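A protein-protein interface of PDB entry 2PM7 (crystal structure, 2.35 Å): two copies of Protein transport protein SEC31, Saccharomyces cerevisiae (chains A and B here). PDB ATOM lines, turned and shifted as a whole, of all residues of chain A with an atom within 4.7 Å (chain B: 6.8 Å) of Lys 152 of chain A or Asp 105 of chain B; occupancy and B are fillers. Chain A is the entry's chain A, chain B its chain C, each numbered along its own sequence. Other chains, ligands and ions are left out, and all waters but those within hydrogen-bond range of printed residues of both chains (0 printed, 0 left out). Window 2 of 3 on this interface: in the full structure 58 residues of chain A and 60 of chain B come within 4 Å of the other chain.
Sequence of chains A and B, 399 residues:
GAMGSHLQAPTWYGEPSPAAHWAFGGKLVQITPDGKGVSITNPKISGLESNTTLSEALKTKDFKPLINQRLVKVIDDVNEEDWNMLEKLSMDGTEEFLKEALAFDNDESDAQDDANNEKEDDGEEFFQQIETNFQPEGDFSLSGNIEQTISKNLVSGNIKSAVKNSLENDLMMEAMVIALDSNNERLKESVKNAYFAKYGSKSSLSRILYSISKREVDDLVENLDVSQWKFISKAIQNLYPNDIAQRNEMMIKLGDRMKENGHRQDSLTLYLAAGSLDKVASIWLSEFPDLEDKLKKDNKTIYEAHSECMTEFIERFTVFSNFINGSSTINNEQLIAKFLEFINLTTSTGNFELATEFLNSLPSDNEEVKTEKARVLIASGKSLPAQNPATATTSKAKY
The side-chain amide nitrogen (NE2) of Gln 148 of chain A sits close to the side-chain amide nitrogen (NE2) of Gln 228 of chain B (3.4 Å). NZ of Lys 152 of chain A is in salt-bridge range of OD2 of Asp 105 of chain B (3.7 Å).
Among the printed residues, pairs that only touch across the chains: Ser 151 of chain A with Ile 208 of chain B, Ser 151 of chain A with Phe 231 of chain B, Lys 152 of chain A with Phe 104 of chain B, Lys 152 of chain A with Phe 231 of chain B, Val 155 of chain A with Phe 231 of chain B, Val 155 of chain A with Lys 234 of chain B and Ser 156 of chain A with Lys 234 of chain B.
Of the printed residues of chain B, Ser 151 of chain A touches Ile 208 and Phe 231. Of chain B, only Phe 104, Asp 105 and Phe 231 come within 4 Å of Lys 152 of chain A. Asn 153 of chain A touches none of the printed residues of chain B. Asp 105 of chain B touches just one residue of chain A: Lys 152 (3.7 Å). Of the printed residues of chain A, Ile 208 of chain B touches Ser 151 (3.5 Å). Of the printed residues of chain A, Gln 228 of chain B touches Gln 148 (3.4 Å). The nearest printed residue of chain A that does not touch Asp 105 of chain B is Gln 148 of chain A (7.4 Å). The nearest printed residue of chain A that does not touch Gln 228 of chain B is Lys 152 of chain A (4.6 Å).
Of the 9 printed residues of chain A, 5 touch a printed residue of chain B. Among the printed residues, Asp or Glu carboxylates within 4 Å of a Lys or Arg side-chain nitrogen of the other chain: Lys 152 of chain A with Asp 105 of chain B (3.7 Å).
No position is printed for both chains. Of the 9 pairs that touch across the chains among the printed residues, none has its exchanged pair printed and touching as well.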
ATOM      1  N   GLN A 148      27.208   2.738  14.819  1.00  0.00           N
ATOM      2  CA  GLN A 148      25.868   3.192  15.177  1.00  0.00           C
ATOM      3  C   GLN A 148      24.764   2.514  14.377  1.00  0.00           C
ATOM      4  O   GLN A 148      23.750   2.095  14.938  1.00  0.00           O
ATOM      5  CB  GLN A 148      25.785   4.710  15.025  1.00  0.00           C
ATOM      6  CG  GLN A 148      26.715   5.435  15.983  1.00  0.00           C
ATOM      7  CD  GLN A 148      26.673   6.939  15.839  1.00  0.00           C
ATOM      8  OE1 GLN A 148      27.051   7.486  14.802  1.00  0.00           O
ATOM      9  NE2 GLN A 148      26.217   7.621  16.884  1.00  0.00           N
ATOM     10  N   THR A 149      24.957   2.392  13.070  1.00  0.00           N
ATOM     11  CA  THR A 149      23.958   1.745  12.234  1.00  0.00           C
ATOM     12  C   THR A 149      23.762   0.298  12.678  1.00  0.00           C
ATOM     13  O   THR A 149      22.640  -0.110  12.979  1.00  0.00           O
ATOM     14  CB  THR A 149      24.366   1.763  10.752  1.00  0.00           C
ATOM     15  OG1 THR A 149      24.557   3.118  10.327  1.00  0.00           O
ATOM     16  CG2 THR A 149      23.285   1.115   9.899  1.00  0.00           C
ATOM     17  N   ILE A 150      24.852  -0.469  12.729  1.00  0.00           N
ATOM     18  CA  ILE A 150      24.792  -1.876  13.143  1.00  0.00           C
ATOM     19  C   ILE A 150      24.222  -2.025  14.551  1.00  0.00           C
ATOM     20  O   ILE A 150      23.365  -2.872  14.789  1.00  0.00           O
ATOM     21  CB  ILE A 150      26.190  -2.541  13.107  1.00  0.00           C
ATOM     22  CG1 ILE A 150      26.709  -2.569  11.669  1.00  0.00           C
ATOM     23  CG2 ILE A 150      26.113  -3.964  13.674  1.00  0.00           C
ATOM     24  CD1 ILE A 150      28.060  -3.203  11.526  1.00  0.00           C
ATOM     25  N   SER A 151      24.708  -1.205  15.477  1.00  0.00           N
ATOM     26  CA  SER A 151      24.231  -1.235  16.854  1.00  0.00           C
ATOM     27  C   SER A 151      22.708  -1.114  16.881  1.00  0.00           C
ATOM     28  O   SER A 151      22.013  -1.943  17.476  1.00  0.00           O
ATOM     29  CB  SER A 151      24.842  -0.081  17.648  1.00  0.00           C
ATOM     30  OG  SER A 151      26.249  -0.190  17.726  1.00  0.00           O
ATOM     31  N   LYS A 152      22.190  -0.074  16.234  1.00  0.00           N
ATOM     32  CA  LYS A 152      20.753   0.148  16.188  1.00  0.00           C
ATOM     33  C   LYS A 152      20.024  -1.076  15.655  1.00  0.00           C
ATOM     34  O   LYS A 152      18.995  -1.461  16.193  1.00  0.00           O
ATOM     35  CB  LYS A 152      20.420   1.369  15.326  1.00  0.00           C
ATOM     36  CG  LYS A 152      20.892   2.690  15.911  1.00  0.00           C
ATOM     37  CD  LYS A 152      20.530   3.865  14.998  1.00  0.00           C
ATOM     38  CE  LYS A 152      21.077   5.189  15.533  1.00  0.00           C
ATOM     39  NZ  LYS A 152      20.819   6.329  14.601  1.00  0.00           N
ATOM     40  N   ASN A 153      20.560  -1.692  14.607  1.00  0.00           N
ATOM     41  CA  ASN A 153      19.934  -2.880  14.030  1.00  0.00           C
ATOM     42  C   ASN A 153      19.810  -3.978  15.079  1.00  0.00           C
ATOM     43  O   ASN A 153      18.777  -4.638  15.194  1.00  0.00           O
ATOM     44  CB  ASN A 153      20.757  -3.416  12.855  1.00  0.00           C
ATOM     45  CG  ASN A 153      20.994  -2.376  11.786  1.00  0.00           C
ATOM     46  OD1 ASN A 153      20.140  -1.530  11.524  1.00  0.00           O
ATOM     47  ND2 ASN A 153      22.154  -2.443  11.146  1.00  0.00           N
ATOM     48  N   LEU A 154      20.877  -4.173  15.840  1.00  0.00           N
ATOM     49  CA  LEU A 154      20.886  -5.191  16.872  1.00  0.00           C
ATOM     50  C   LEU A 154      19.720  -5.003  17.835  1.00  0.00           C
ATOM     51  O   LEU A 154      18.819  -5.840  17.893  1.00  0.00           O
ATOM     52  CB  LEU A 154      22.217  -5.146  17.620  1.00  0.00           C
ATOM     53  CG  LEU A 154      23.399  -5.552  16.735  1.00  0.00           C
ATOM     54  CD1 LEU A 154      24.708  -5.330  17.456  1.00  0.00           C
ATOM     55  CD2 LEU A 154      23.242  -7.011  16.341  1.00  0.00           C
ATOM     56  N   VAL A 155      19.733  -3.899  18.577  1.00  0.00           N
ATOM     57  CA  VAL A 155      18.671  -3.617  19.532  1.00  0.00           C
ATOM     58  C   VAL A 155      17.271  -3.678  18.918  1.00  0.00           C
ATOM     59  O   VAL A 155      16.344  -4.228  19.515  1.00  0.00           O
ATOM     60  CB  VAL A 155      18.866  -2.254  20.167  1.00  0.00           C
ATOM     61  CG1 VAL A 155      17.661  -1.910  21.003  1.00  0.00           C
ATOM     62  CG2 VAL A 155      20.099  -2.277  21.032  1.00  0.00           C
ATOM     63  N   SER A 156      17.111  -3.106  17.731  1.00  0.00           N
ATOM     64  CA  SER A 156      15.821  -3.140  17.061  1.00  0.00           C
ATOM     65  C   SER A 156      15.489  -4.587  16.707  1.00  0.00           C
ATOM     66  O   SER A 156      14.640  -4.848  15.851  1.00  0.00           O
ATOM     67  CB  SER A 156      15.861  -2.298  15.787  1.00  0.00           C
ATOM     68  OG  SER A 156      14.680  -2.478  15.028  1.00  0.00           O
ATOM     69  N   ALA B 103      12.088   7.799  19.658  1.00  0.00           N
ATOM     70  CA  ALA B 103      12.352   7.346  18.296  1.00  0.00           C
ATOM     71  C   ALA B 103      13.681   7.866  17.747  1.00  0.00           C
ATOM     72  O   ALA B 103      14.237   8.842  18.254  1.00  0.00           O
ATOM     73  CB  ALA B 103      11.212   7.774  17.379  1.00  0.00           C
ATOM     74  N   PHE B 104      14.182   7.209  16.704  1.00  0.00           N
ATOM     75  CA  PHE B 104      15.440   7.604  16.084  1.00  0.00           C
ATOM     76  C   PHE B 104      15.242   8.682  15.028  1.00  0.00           C
ATOM     77  O   PHE B 104      14.113   9.041  14.695  1.00  0.00           O
ATOM     78  CB  PHE B 104      16.130   6.392  15.454  1.00  0.00           C
ATOM     79  CG  PHE B 104      16.536   5.344  16.449  1.00  0.00           C
ATOM     80  CD1 PHE B 104      15.613   4.409  16.909  1.00  0.00           C
ATOM     81  CD2 PHE B 104      17.835   5.306  16.944  1.00  0.00           C
ATOM     82  CE1 PHE B 104      15.981   3.448  17.851  1.00  0.00           C
ATOM     83  CE2 PHE B 104      18.215   4.350  17.887  1.00  0.00           C
ATOM     84  CZ  PHE B 104      17.286   3.420  18.341  1.00  0.00           C
ATOM     85  N   ASP B 105      16.353   9.191  14.507  1.00  0.00           N
ATOM     86  CA  ASP B 105      16.333  10.239  13.489  1.00  0.00           C
ATOM     87  C   ASP B 105      15.502   9.835  12.275  1.00  0.00           C
ATOM     88  O   ASP B 105      16.048   9.496  11.225  1.00  0.00           O
ATOM     89  CB  ASP B 105      17.764  10.546  13.053  1.00  0.00           C
ATOM     90  CG  ASP B 105      18.704  10.698  14.230  1.00  0.00           C
ATOM     91  OD1 ASP B 105      18.513  11.647  15.024  1.00  0.00           O
ATOM     92  OD2 ASP B 105      19.625   9.861  14.363  1.00  0.00           O
ATOM     93  N   ILE B 208      29.399  -3.683  22.539  1.00  0.00           N
ATOM     94  CA  ILE B 208      27.951  -3.685  22.492  1.00  0.00           C
ATOM     95  C   ILE B 208      27.450  -5.080  22.178  1.00  0.00           C
ATOM     96  O   ILE B 208      26.520  -5.563  22.808  1.00  0.00           O
ATOM     97  CB  ILE B 208      27.440  -2.663  21.443  1.00  0.00           C
ATOM     98  CG1 ILE B 208      27.344  -1.286  22.106  1.00  0.00           C
ATOM     99  CG2 ILE B 208      26.103  -3.101  20.856  1.00  0.00           C
ATOM    100  CD1 ILE B 208      26.792  -0.221  21.232  1.00  0.00           C
ATOM    101  N   GLN B 228      24.125   8.624  23.263  1.00  0.00           N
ATOM    102  CA  GLN B 228      23.472   7.534  22.556  1.00  0.00           C
ATOM    103  C   GLN B 228      22.361   6.957  23.441  1.00  0.00           C
ATOM    104  O   GLN B 228      21.949   5.809  23.268  1.00  0.00           O
ATOM    105  CB  GLN B 228      24.516   6.466  22.207  1.00  0.00           C
ATOM    106  CG  GLN B 228      24.033   5.308  21.319  1.00  0.00           C
ATOM    107  CD  GLN B 228      23.550   5.744  19.938  1.00  0.00           C
ATOM    108  OE1 GLN B 228      22.424   6.218  19.777  1.00  0.00           O
ATOM    109  NE2 GLN B 228      24.406   5.585  18.937  1.00  0.00           N
ATOM    110  N   LYS B 230      19.188   7.167  23.469  1.00  0.00           N
ATOM    111  CA  LYS B 230      18.031   6.573  22.808  1.00  0.00           C
ATOM    112  C   LYS B 230      18.308   5.124  22.413  1.00  0.00           C
ATOM    113  O   LYS B 230      17.391   4.314  22.267  1.00  0.00           O
ATOM    114  CB  LYS B 230      17.635   7.378  21.567  1.00  0.00           C
ATOM    115  CG  LYS B 230      17.056   8.747  21.877  1.00  0.00           C
ATOM    116  CD  LYS B 230      16.451   9.387  20.635  1.00  0.00           C
ATOM    117  CE  LYS B 230      15.866  10.753  20.954  1.00  0.00           C
ATOM    118  NZ  LYS B 230      15.127  11.314  19.798  1.00  0.00           N
ATOM    119  N   PHE B 231      19.580   4.797  22.236  1.00  0.00           N
ATOM    120  CA  PHE B 231      19.953   3.440  21.874  1.00  0.00           C
ATOM    121  C   PHE B 231      19.845   2.561  23.114  1.00  0.00           C
ATOM    122  O   PHE B 231      19.348   1.435  23.058  1.00  0.00           O
ATOM    123  CB  PHE B 231      21.383   3.402  21.351  1.00  0.00           C
ATOM    124  CG  PHE B 231      21.863   2.028  21.048  1.00  0.00           C
ATOM    125  CD1 PHE B 231      21.345   1.324  19.970  1.00  0.00           C
ATOM    126  CD2 PHE B 231      22.800   1.415  21.867  1.00  0.00           C
ATOM    127  CE1 PHE B 231      21.753   0.025  19.707  1.00  0.00           C
ATOM    128  CE2 PHE B 231      23.216   0.111  21.615  1.00  0.00           C
ATOM    129  CZ  PHE B 231      22.690  -0.586  20.532  1.00  0.00           C
ATOM    130  N   LYS B 234      16.095   2.020  23.889  1.00  0.00           N
ATOM    131  CA  LYS B 234      15.564   1.009  22.988  1.00  0.00           C
ATOM    132  C   LYS B 234      16.116  -0.371  23.363  1.00  0.00           C
ATOM    133  O   LYS B 234      15.422  -1.376  23.248  1.00  0.00           O
ATOM    134  CB  LYS B 234      15.921   1.378  21.544  1.00  0.00           C
ATOM    135  CG  LYS B 234      15.438   0.400  20.480  1.00  0.00           C
ATOM    136  CD  LYS B 234      13.928   0.186  20.469  1.00  0.00           C
ATOM    137  CE  LYS B 234      13.550  -0.829  19.383  1.00  0.00           C
ATOM    138  NZ  LYS B 234      12.110  -1.221  19.383  1.00  0.00           N
